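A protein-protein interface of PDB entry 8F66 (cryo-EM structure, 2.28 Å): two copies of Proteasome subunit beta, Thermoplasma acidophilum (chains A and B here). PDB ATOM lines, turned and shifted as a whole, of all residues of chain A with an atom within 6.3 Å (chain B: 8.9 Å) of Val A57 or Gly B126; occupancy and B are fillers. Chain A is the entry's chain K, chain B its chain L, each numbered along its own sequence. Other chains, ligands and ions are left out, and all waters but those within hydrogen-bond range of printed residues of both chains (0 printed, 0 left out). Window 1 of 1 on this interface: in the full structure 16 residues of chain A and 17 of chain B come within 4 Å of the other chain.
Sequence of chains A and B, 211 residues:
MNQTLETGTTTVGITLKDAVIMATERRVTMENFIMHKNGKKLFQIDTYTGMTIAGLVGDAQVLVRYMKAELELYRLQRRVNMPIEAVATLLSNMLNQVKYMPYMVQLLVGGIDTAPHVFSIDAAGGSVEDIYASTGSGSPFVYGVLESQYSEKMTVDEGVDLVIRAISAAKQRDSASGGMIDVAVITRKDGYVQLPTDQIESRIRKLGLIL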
ATOM      1  N   VAL A  28     -12.415 -20.280 -12.768  1.00  0.00           N
ATOM      2  CA  VAL A  28     -12.133 -21.697 -12.975  1.00  0.00           C
ATOM      3  C   VAL A  28     -12.121 -22.379 -11.615  1.00  0.00           C
ATOM      4  O   VAL A  28     -11.411 -21.941 -10.701  1.00  0.00           O
ATOM      5  CB  VAL A  28     -10.796 -21.914 -13.702  1.00  0.00           C
ATOM      6  CG1 VAL A  28     -10.543 -23.399 -13.911  1.00  0.00           C
ATOM      7  CG2 VAL A  28     -10.779 -21.174 -15.031  1.00  0.00           C
ATOM      8  N   THR A  29     -12.903 -23.447 -11.480  1.00  0.00           N
ATOM      9  CA  THR A  29     -12.905 -24.260 -10.270  1.00  0.00           C
ATOM     10  C   THR A  29     -12.185 -25.574 -10.552  1.00  0.00           C
ATOM     11  O   THR A  29     -12.527 -26.283 -11.505  1.00  0.00           O
ATOM     12  CB  THR A  29     -14.332 -24.520  -9.786  1.00  0.00           C
ATOM     13  OG1 THR A  29     -15.026 -25.330 -10.742  1.00  0.00           O
ATOM     14  CG2 THR A  29     -15.081 -23.209  -9.599  1.00  0.00           C
ATOM     15  N   MET A  30     -11.192 -25.894  -9.726  1.00  0.00           N
ATOM     16  CA  MET A  30     -10.395 -27.103  -9.885  1.00  0.00           C
ATOM     17  C   MET A  30     -10.107 -27.678  -8.508  1.00  0.00           C
ATOM     18  O   MET A  30      -9.642 -26.954  -7.623  1.00  0.00           O
ATOM     19  CB  MET A  30      -9.090 -26.808 -10.632  1.00  0.00           C
ATOM     20  CG  MET A  30      -8.521 -27.986 -11.399  1.00  0.00           C
ATOM     21  SD  MET A  30      -7.089 -27.522 -12.390  1.00  0.00           S
ATOM     22  CE  MET A  30      -7.861 -26.523 -13.658  1.00  0.00           C
ATOM     23  N   ILE A  53     -15.642 -22.339 -24.608  1.00  0.00           N
ATOM     24  CA  ILE A  53     -15.580 -23.677 -24.038  1.00  0.00           C
ATOM     25  C   ILE A  53     -16.199 -23.671 -22.648  1.00  0.00           C
ATOM     26  O   ILE A  53     -15.950 -22.763 -21.846  1.00  0.00           O
ATOM     27  CB  ILE A  53     -14.127 -24.197 -23.982  1.00  0.00           C
ATOM     28  CG1 ILE A  53     -13.198 -23.131 -23.395  1.00  0.00           C
ATOM     29  CG2 ILE A  53     -13.656 -24.616 -25.367  1.00  0.00           C
ATOM     30  CD1 ILE A  53     -12.025 -23.694 -22.630  1.00  0.00           C
ATOM     31  N   GLY A  55     -17.262 -26.714 -19.447  1.00  0.00           N
ATOM     32  CA  GLY A  55     -17.123 -28.093 -19.022  1.00  0.00           C
ATOM     33  C   GLY A  55     -15.749 -28.417 -18.471  1.00  0.00           C
ATOM     34  O   GLY A  55     -15.128 -27.582 -17.807  1.00  0.00           O
ATOM     35  N   LEU A  56     -15.265 -29.628 -18.736  1.00  0.00           N
ATOM     36  CA  LEU A  56     -13.954 -30.035 -18.245  1.00  0.00           C
ATOM     37  C   LEU A  56     -12.854 -29.276 -18.976  1.00  0.00           C
ATOM     38  O   LEU A  56     -12.864 -29.175 -20.205  1.00  0.00           O
ATOM     39  CB  LEU A  56     -13.767 -31.542 -18.419  1.00  0.00           C
ATOM     40  CG  LEU A  56     -12.519 -32.141 -17.766  1.00  0.00           C
ATOM     41  CD1 LEU A  56     -12.790 -32.494 -16.312  1.00  0.00           C
ATOM     42  CD2 LEU A  56     -12.038 -33.362 -18.534  1.00  0.00           C
ATOM     43  N   VAL A  57     -11.902 -28.739 -18.209  1.00  0.00           N
ATOM     44  CA  VAL A  57     -10.849 -27.908 -18.788  1.00  0.00           C
ATOM     45  C   VAL A  57      -9.945 -28.737 -19.692  1.00  0.00           C
ATOM     46  O   VAL A  57      -9.552 -28.297 -20.778  1.00  0.00           O
ATOM     47  CB  VAL A  57     -10.047 -27.208 -17.674  1.00  0.00           C
ATOM     48  CG1 VAL A  57      -8.946 -26.345 -18.270  1.00  0.00           C
ATOM     49  CG2 VAL A  57     -10.970 -26.374 -16.803  1.00  0.00           C
ATOM     50  N   GLY A  58      -9.600 -29.951 -19.256  1.00  0.00           N
ATOM     51  CA  GLY A  58      -8.667 -30.765 -20.019  1.00  0.00           C
ATOM     52  C   GLY A  58      -9.185 -31.132 -21.395  1.00  0.00           C
ATOM     53  O   GLY A  58      -8.471 -31.018 -22.394  1.00  0.00           O
ATOM     54  N   ASP A  59     -10.439 -31.584 -21.468  1.00  0.00           N
ATOM     55  CA  ASP A  59     -11.024 -31.943 -22.756  1.00  0.00           C
ATOM     56  C   ASP A  59     -11.176 -30.717 -23.651  1.00  0.00           C
ATOM     57  O   ASP A  59     -10.935 -30.783 -24.863  1.00  0.00           O
ATOM     58  CB  ASP A  59     -12.375 -32.629 -22.551  1.00  0.00           C
ATOM     59  CG  ASP A  59     -12.239 -34.021 -21.974  1.00  0.00           C
ATOM     60  OD1 ASP A  59     -11.126 -34.583 -22.033  1.00  0.00           O
ATOM     61  OD2 ASP A  59     -13.244 -34.557 -21.462  1.00  0.00           O
ATOM     62  N   ALA A  60     -11.584 -29.589 -23.067  1.00  0.00           N
ATOM     63  CA  ALA A  60     -11.823 -28.384 -23.855  1.00  0.00           C
ATOM     64  C   ALA A  60     -10.535 -27.866 -24.486  1.00  0.00           C
ATOM     65  O   ALA A  60     -10.521 -27.470 -25.657  1.00  0.00           O
ATOM     66  CB  ALA A  60     -12.467 -27.310 -22.978  1.00  0.00           C
ATOM     67  N   GLN A  61      -9.439 -27.860 -23.722  1.00  0.00           N
ATOM     68  CA  GLN A  61      -8.180 -27.337 -24.244  1.00  0.00           C
ATOM     69  C   GLN A  61      -7.632 -28.211 -25.366  1.00  0.00           C
ATOM     70  O   GLN A  61      -7.031 -27.702 -26.318  1.00  0.00           O
ATOM     71  CB  GLN A  61      -7.156 -27.205 -23.115  1.00  0.00           C
ATOM     72  CG  GLN A  61      -7.488 -26.116 -22.109  1.00  0.00           C
ATOM     73  CD  GLN A  61      -6.551 -26.113 -20.918  1.00  0.00           C
ATOM     74  OE1 GLN A  61      -6.141 -27.168 -20.435  1.00  0.00           O
ATOM     75  NE2 GLN A  61      -6.209 -24.925 -20.437  1.00  0.00           N
ATOM     76  N   VAL A  62      -7.823 -29.528 -25.267  1.00  0.00           N
ATOM     77  CA  VAL A  62      -7.389 -30.424 -26.335  1.00  0.00           C
ATOM     78  C   VAL A  62      -8.159 -30.135 -27.619  1.00  0.00           C
ATOM     79  O   VAL A  62      -7.581 -30.101 -28.712  1.00  0.00           O
ATOM     80  CB  VAL A  62      -7.541 -31.890 -25.890  1.00  0.00           C
ATOM     81  CG1 VAL A  62      -7.581 -32.820 -27.095  1.00  0.00           C
ATOM     82  CG2 VAL A  62      -6.409 -32.280 -24.955  1.00  0.00           C
ATOM     83  N   MET A 104     -16.432 -34.151 -22.220  1.00  0.00           N
ATOM     84  CA  MET A 104     -17.454 -33.565 -21.352  1.00  0.00           C
ATOM     85  C   MET A 104     -17.406 -32.047 -21.505  1.00  0.00           C
ATOM     86  O   MET A 104     -16.975 -31.309 -20.616  1.00  0.00           O
ATOM     87  CB  MET A 104     -17.244 -33.999 -19.908  1.00  0.00           C
ATOM     88  CG  MET A 104     -16.896 -35.468 -19.750  1.00  0.00           C
ATOM     89  SD  MET A 104     -18.349 -36.535 -19.734  1.00  0.00           S
ATOM     90  CE  MET A 104     -19.179 -35.955 -18.256  1.00  0.00           C
ATOM     91  N   ALA B  88       3.910 -27.085 -20.097  1.00  0.00           N
ATOM     92  CA  ALA B  88       2.570 -27.372 -19.597  1.00  0.00           C
ATOM     93  C   ALA B  88       1.681 -27.967 -20.679  1.00  0.00           C
ATOM     94  O   ALA B  88       0.858 -28.843 -20.391  1.00  0.00           O
ATOM     95  CB  ALA B  88       1.940 -26.103 -19.024  1.00  0.00           C
ATOM     96  N   THR B  89       1.824 -27.503 -21.923  1.00  0.00           N
ATOM     97  CA  THR B  89       1.029 -28.051 -23.017  1.00  0.00           C
ATOM     98  C   THR B  89       1.361 -29.517 -23.264  1.00  0.00           C
ATOM     99  O   THR B  89       0.462 -30.332 -23.500  1.00  0.00           O
ATOM    100  CB  THR B  89       1.246 -27.230 -24.289  1.00  0.00           C
ATOM    101  OG1 THR B  89       1.031 -25.843 -24.005  1.00  0.00           O
ATOM    102  CG2 THR B  89       0.283 -27.670 -25.383  1.00  0.00           C
ATOM    103  N   LEU B  91       2.562 -31.674 -21.046  1.00  0.00           N
ATOM    104  CA  LEU B  91       1.995 -32.426 -19.931  1.00  0.00           C
ATOM    105  C   LEU B  91       0.484 -32.562 -20.071  1.00  0.00           C
ATOM    106  O   LEU B  91      -0.088 -33.608 -19.742  1.00  0.00           O
ATOM    107  CB  LEU B  91       2.346 -31.752 -18.606  1.00  0.00           C
ATOM    108  CG  LEU B  91       3.462 -32.400 -17.785  1.00  0.00           C
ATOM    109  CD1 LEU B  91       3.900 -31.481 -16.656  1.00  0.00           C
ATOM    110  CD2 LEU B  91       3.017 -33.749 -17.245  1.00  0.00           C
ATOM    111  N   SER B  92      -0.180 -31.509 -20.553  1.00  0.00           N
ATOM    112  CA  SER B  92      -1.628 -31.548 -20.719  1.00  0.00           C
ATOM    113  C   SER B  92      -2.045 -32.628 -21.709  1.00  0.00           C
ATOM    114  O   SER B  92      -3.033 -33.338 -21.486  1.00  0.00           O
ATOM    115  CB  SER B  92      -2.135 -30.178 -21.173  1.00  0.00           C
ATOM    116  OG  SER B  92      -3.411 -30.279 -21.779  1.00  0.00           O
ATOM    117  N   ASN B  93      -1.306 -32.764 -22.812  1.00  0.00           N
ATOM    118  CA  ASN B  93      -1.647 -33.764 -23.819  1.00  0.00           C
ATOM    119  C   ASN B  93      -1.500 -35.178 -23.267  1.00  0.00           C
ATOM    120  O   ASN B  93      -2.354 -36.040 -23.506  1.00  0.00           O
ATOM    121  CB  ASN B  93      -0.775 -33.576 -25.060  1.00  0.00           C
ATOM    122  CG  ASN B  93      -1.213 -32.398 -25.906  1.00  0.00           C
ATOM    123  OD1 ASN B  93      -2.399 -32.223 -26.179  1.00  0.00           O
ATOM    124  ND2 ASN B  93      -0.254 -31.583 -26.330  1.00  0.00           N
ATOM    125  N   LEU B  95      -1.636 -36.292 -20.118  1.00  0.00           N
ATOM    126  CA  LEU B  95      -2.629 -36.634 -19.104  1.00  0.00           C
ATOM    127  C   LEU B  95      -4.016 -36.804 -19.714  1.00  0.00           C
ATOM    128  O   LEU B  95      -4.775 -37.690 -19.303  1.00  0.00           O
ATOM    129  CB  LEU B  95      -2.648 -35.572 -18.006  1.00  0.00           C
ATOM    130  CG  LEU B  95      -1.355 -35.438 -17.197  1.00  0.00           C
ATOM    131  CD1 LEU B  95      -1.330 -34.131 -16.430  1.00  0.00           C
ATOM    132  CD2 LEU B  95      -1.186 -36.617 -16.256  1.00  0.00           C
ATOM    133  N   ASN B  96      -4.367 -35.967 -20.693  1.00  0.00           N
ATOM    134  CA  ASN B  96      -5.691 -36.058 -21.299  1.00  0.00           C
ATOM    135  C   ASN B  96      -5.833 -37.295 -22.179  1.00  0.00           C
ATOM    136  O   ASN B  96      -6.949 -37.789 -22.373  1.00  0.00           O
ATOM    137  CB  ASN B  96      -5.988 -34.796 -22.108  1.00  0.00           C
ATOM    138  CG  ASN B  96      -7.452 -34.677 -22.484  1.00  0.00           C
ATOM    139  OD1 ASN B  96      -7.853 -35.050 -23.585  1.00  0.00           O
ATOM    140  ND2 ASN B  96      -8.259 -34.157 -21.568  1.00  0.00           N
ATOM    141  N   LYS B  99      -7.184 -40.046 -19.938  1.00  0.00           N
ATOM    142  CA  LYS B  99      -8.038 -39.463 -18.906  1.00  0.00           C
ATOM    143  C   LYS B  99      -8.964 -40.488 -18.259  1.00  0.00           C
ATOM    144  O   LYS B  99      -9.356 -40.321 -17.098  1.00  0.00           O
ATOM    145  CB  LYS B  99      -8.851 -38.306 -19.491  1.00  0.00           C
ATOM    146  CG  LYS B  99      -9.977 -38.727 -20.420  1.00  0.00           C
ATOM    147  CD  LYS B  99     -10.444 -37.565 -21.277  1.00  0.00           C
ATOM    148  CE  LYS B  99     -10.663 -37.991 -22.718  1.00  0.00           C
ATOM    149  NZ  LYS B  99     -10.350 -36.894 -23.677  1.00  0.00           N
ATOM    150  N   VAL B 105      -2.707 -37.413 -10.065  1.00  0.00           N
ATOM    151  CA  VAL B 105      -1.705 -36.434  -9.661  1.00  0.00           C
ATOM    152  C   VAL B 105      -2.257 -35.027  -9.847  1.00  0.00           C
ATOM    153  O   VAL B 105      -3.186 -34.794 -10.623  1.00  0.00           O
ATOM    154  CB  VAL B 105      -0.385 -36.587 -10.458  1.00  0.00           C
ATOM    155  CG1 VAL B 105       0.216 -37.968 -10.254  1.00  0.00           C
ATOM    156  CG2 VAL B 105      -0.625 -36.313 -11.935  1.00  0.00           C
ATOM    157  N   GLN B 106      -1.671 -34.083  -9.112  1.00  0.00           N
ATOM    158  CA  GLN B 106      -1.841 -32.657  -9.342  1.00  0.00           C
ATOM    159  C   GLN B 106      -0.455 -32.037  -9.412  1.00  0.00           C
ATOM    160  O   GLN B 106       0.375 -32.272  -8.528  1.00  0.00           O
ATOM    161  CB  GLN B 106      -2.677 -31.998  -8.239  1.00  0.00           C
ATOM    162  CG  GLN B 106      -4.105 -32.516  -8.151  1.00  0.00           C
ATOM    163  CD  GLN B 106      -4.229 -33.749  -7.279  1.00  0.00           C
ATOM    164  OE1 GLN B 106      -3.500 -33.906  -6.299  1.00  0.00           O
ATOM    165  NE2 GLN B 106      -5.156 -34.632  -7.632  1.00  0.00           N
ATOM    166  N   LEU B 107      -0.201 -31.247 -10.452  1.00  0.00           N
ATOM    167  CA  LEU B 107       1.150 -30.815 -10.777  1.00  0.00           C
ATOM    168  C   LEU B 107       1.243 -29.299 -10.848  1.00  0.00           C
ATOM    169  O   LEU B 107       0.281 -28.621 -11.224  1.00  0.00           O
ATOM    170  CB  LEU B 107       1.613 -31.418 -12.109  1.00  0.00           C
ATOM    171  CG  LEU B 107       1.456 -32.931 -12.257  1.00  0.00           C
ATOM    172  CD1 LEU B 107       1.593 -33.351 -13.711  1.00  0.00           C
ATOM    173  CD2 LEU B 107       2.467 -33.660 -11.387  1.00  0.00           C
ATOM    174  N   PHE B 119       2.341 -22.740 -13.782  1.00  0.00           N
ATOM    175  CA  PHE B 119       1.213 -23.427 -14.392  1.00  0.00           C
ATOM    176  C   PHE B 119       0.688 -24.501 -13.450  1.00  0.00           C
ATOM    177  O   PHE B 119       1.466 -25.211 -12.806  1.00  0.00           O
ATOM    178  CB  PHE B 119       1.603 -24.063 -15.732  1.00  0.00           C
ATOM    179  CG  PHE B 119       1.653 -23.090 -16.876  1.00  0.00           C
ATOM    180  CD1 PHE B 119       2.812 -22.381 -17.150  1.00  0.00           C
ATOM    181  CD2 PHE B 119       0.543 -22.886 -17.678  1.00  0.00           C
ATOM    182  CE1 PHE B 119       2.863 -21.489 -18.206  1.00  0.00           C
ATOM    183  CE2 PHE B 119       0.587 -21.993 -18.735  1.00  0.00           C
ATOM    184  CZ  PHE B 119       1.749 -21.293 -18.997  1.00  0.00           C
ATOM    185  N   SER B 120      -0.634 -24.615 -13.376  1.00  0.00           N
ATOM    186  CA  SER B 120      -1.294 -25.655 -12.602  1.00  0.00           C
ATOM    187  C   SER B 120      -1.997 -26.616 -13.552  1.00  0.00           C
ATOM    188  O   SER B 120      -2.777 -26.188 -14.408  1.00  0.00           O
ATOM    189  CB  SER B 120      -2.296 -25.051 -11.616  1.00  0.00           C
ATOM    190  OG  SER B 120      -2.747 -26.022 -10.690  1.00  0.00           O
ATOM    191  N   ILE B 121      -1.717 -27.907 -13.402  1.00  0.00           N
ATOM    192  CA  ILE B 121      -2.262 -28.937 -14.278  1.00  0.00           C
ATOM    193  C   ILE B 121      -2.930 -30.001 -13.420  1.00  0.00           C
ATOM    194  O   ILE B 121      -2.330 -30.497 -12.459  1.00  0.00           O
ATOM    195  CB  ILE B 121      -1.179 -29.569 -15.176  1.00  0.00           C
ATOM    196  CG1 ILE B 121      -0.411 -28.495 -15.952  1.00  0.00           C
ATOM    197  CG2 ILE B 121      -1.808 -30.550 -16.147  1.00  0.00           C
ATOM    198  CD1 ILE B 121       0.868 -28.034 -15.285  1.00  0.00           C
ATOM    199  N   ASP B 122      -4.165 -30.353 -13.764  1.00  0.00           N
ATOM    200  CA  ASP B 122      -4.919 -31.372 -13.051  1.00  0.00           C
ATOM    201  C   ASP B 122      -4.748 -32.736 -13.715  1.00  0.00           C
ATOM    202  O   ASP B 122      -4.012 -32.898 -14.691  1.00  0.00           O
ATOM    203  CB  ASP B 122      -6.403 -30.987 -12.964  1.00  0.00           C
ATOM    204  CG  ASP B 122      -7.066 -30.859 -14.326  1.00  0.00           C
ATOM    205  OD1 ASP B 122      -7.149 -31.863 -15.064  1.00  0.00           O
ATOM    206  OD2 ASP B 122      -7.518 -29.744 -14.658  1.00  0.00           O
ATOM    207  N   ALA B 123      -5.450 -33.729 -13.161  1.00  0.00           N
ATOM    208  CA  ALA B 123      -5.316 -35.100 -13.641  1.00  0.00           C
ATOM    209  C   ALA B 123      -5.845 -35.264 -15.061  1.00  0.00           C
ATOM    210  O   ALA B 123      -5.315 -36.073 -15.829  1.00  0.00           O
ATOM    211  CB  ALA B 123      -6.034 -36.058 -12.694  1.00  0.00           C
ATOM    212  N   ALA B 124      -6.881 -34.512 -15.428  1.00  0.00           N
ATOM    213  CA  ALA B 124      -7.482 -34.626 -16.751  1.00  0.00           C
ATOM    214  C   ALA B 124      -6.746 -33.817 -17.812  1.00  0.00           C
ATOM    215  O   ALA B 124      -7.164 -33.822 -18.974  1.00  0.00           O
ATOM    216  CB  ALA B 124      -8.951 -34.198 -16.700  1.00  0.00           C
ATOM    217  N   GLY B 125      -5.666 -33.131 -17.447  1.00  0.00           N
ATOM    218  CA  GLY B 125      -4.903 -32.355 -18.403  1.00  0.00           C
ATOM    219  C   GLY B 125      -5.262 -30.891 -18.491  1.00  0.00           C
ATOM    220  O   GLY B 125      -4.744 -30.198 -19.372  1.00  0.00           O
ATOM    221  N   GLY B 126      -6.134 -30.394 -17.617  1.00  0.00           N
ATOM    222  CA  GLY B 126      -6.458 -28.982 -17.609  1.00  0.00           C
ATOM    223  C   GLY B 126      -5.311 -28.128 -17.109  1.00  0.00           C
ATOM    224  O   GLY B 126      -4.886 -28.269 -15.960  1.00  0.00           O
ATOM    225  N   SER B 127      -4.803 -27.239 -17.958  1.00  0.00           N
ATOM    226  CA  SER B 127      -3.664 -26.391 -17.632  1.00  0.00           C
ATOM    227  C   SER B 127      -4.090 -24.931 -17.679  1.00  0.00           C
ATOM    228  O   SER B 127      -4.751 -24.504 -18.630  1.00  0.00           O
ATOM    229  CB  SER B 127      -2.502 -26.640 -18.597  1.00  0.00           C
ATOM    230  OG  SER B 127      -1.446 -25.723 -18.376  1.00  0.00           O
ATOM    231  N   VAL B 128      -3.713 -24.172 -16.652  1.00  0.00           N
ATOM    232  CA  VAL B 128      -4.057 -22.757 -16.553  1.00  0.00           C
ATOM    233  C   VAL B 128      -2.931 -22.028 -15.831  1.00  0.00           C
ATOM    234  O   VAL B 128      -2.407 -22.511 -14.823  1.00  0.00           O
ATOM    235  CB  VAL B 128      -5.411 -22.558 -15.836  1.00  0.00           C
ATOM    236  CG1 VAL B 128      -5.650 -23.676 -14.836  1.00  0.00           C
ATOM    237  CG2 VAL B 128      -5.484 -21.198 -15.157  1.00  0.00           C
ATOM    238  N   GLU B 129      -2.557 -20.863 -16.356  1.00  0.00           N
ATOM    239  CA  GLU B 129      -1.499 -20.044 -15.778  1.00  0.00           C
ATOM    240  C   GLU B 129      -2.040 -19.187 -14.642  1.00  0.00           C
ATOM    241  O   GLU B 129      -3.189 -18.736 -14.676  1.00  0.00           O
ATOM    242  CB  GLU B 129      -0.868 -19.148 -16.845  1.00  0.00           C
ATOM    243  CG  GLU B 129       0.617 -18.907 -16.657  1.00  0.00           C
ATOM    244  CD  GLU B 129       1.107 -17.681 -17.405  1.00  0.00           C
ATOM    245  OE1 GLU B 129       1.980 -16.964 -16.869  1.00  0.00           O
ATOM    246  OE2 GLU B 129       0.621 -17.435 -18.527  1.00  0.00           O
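The backbone carbonyl oxygen (O) of Gly A58 sits close to the side-chain amide nitrogen (ND2) of Asn B96 (3.3 Å). OE1 of Gln A61 is in hydrogen-bond range of N of Ser B127, 2.8 Å away. The side-chain amide nitrogen of Asn B96 sits at hydrogen-bond distance from the side-chain carboxylate of Asp A59, at 2.9 Å. The side-chain carboxylate (OD1) of Asp A59 lies within salt-bridge range of the side-chain amino group (NZ) of Lys B99 (2.9 Å). SD of Met A30 sits close to OD2 of Asp B122, at 3.2 Å.
N of Gly B125 sits at hydrogen-bond distance from OD1 of Asp B122, 3.1 Å away. The backbone NH (N) of Ser B120 is in hydrogen-bond range of the backbone carbonyl oxygen (O) of Val B128 (3.1 Å). The backbone NH (N) of Ala B124 sits at hydrogen-bond distance from the side-chain carboxylate (OD1) of Asp B122 (2.7 Å). OD1 of Asn B96 sits at hydrogen-bond distance from NZ of Lys B99. The side-chain hydroxyl (OG) of Ser B92 lies within hydrogen-bond range of the backbone carbonyl oxygen (O) of Gly B125. N of Leu A56 lies within hydrogen-bond range of O of Met A104 (3.0 Å).
Among the printed residues, pairs that only touch across the chains: Gln A61 with Gly B126, Val A62 with Asn B96, Gln A61 with Gly B125, Gly A58 with Gly B126, Gly A58 with Ala B124, Val A57 with Gly B126, Leu A56 with Ala B124, Gly A58 with Gly B125 and Met A30 with Val B128.
Of chain B, only Gly B126 (3.7 Å) comes within 4 Å of Val A57. Gly B126 touches just these residues of chain A: Val A57 (3.7 Å), Gly A58 (3.5 Å) and Gln A61 (3.4 Å). Of chain B, only Ala B124 comes within 4 Å of Leu A56. Gly A58 touches four residues of chain B. Of the printed residues of chain B, Asp A59 touches Asn B96 (2.9 Å) and Lys B99 (2.9 Å). Printed residues of chain A within 4 Å of Val B128: Met A30. Of the printed residues of chain A, Asn B96 touches Gly A58, Asp A59 and Val A62. Printed residues of chain B within 4 Å of Met A30: Asp B122 (3.2 Å) and Val B128 (3.8 Å). Ala B123 touches none of the printed residues of chain A. The nearest residue of chain A that does not touch Gly B126 is Met A30 (4.1 Å). The nearest printed residue of chain B that does not touch Val A62 is Asn B93 (4.2 Å).
Printed residues of chain B that touch a printed residue of chain A: Asn B96, Lys B99, Asp B122, Ala B124, Gly B125, Gly B126, Ser B127 and Val B128. Hydrophobic or aromatic side chains of chain B within 4 Å of the printed part of chain A: Ala B124 and Val B128. Of the 13 printed residues of chain A, 7 touch a printed residue of chain B. Hydrophobic or aromatic side chains of chain A that line the printed part of chain B: Met A30, Leu A56, Val A57 and Val A62. Among the printed residues, 14 pairs touch across the chains. Among the printed residues, Asp or Glu carboxylates within 4 Å of a Lys or Arg side-chain nitrogen of the other chain: Asp A59 with Lys B99 (2.9 Å).
No position is printed for both chains. Of the 14 pairs that touch across the chains among the printed residues, none has its exchanged pair printed and touching as well.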
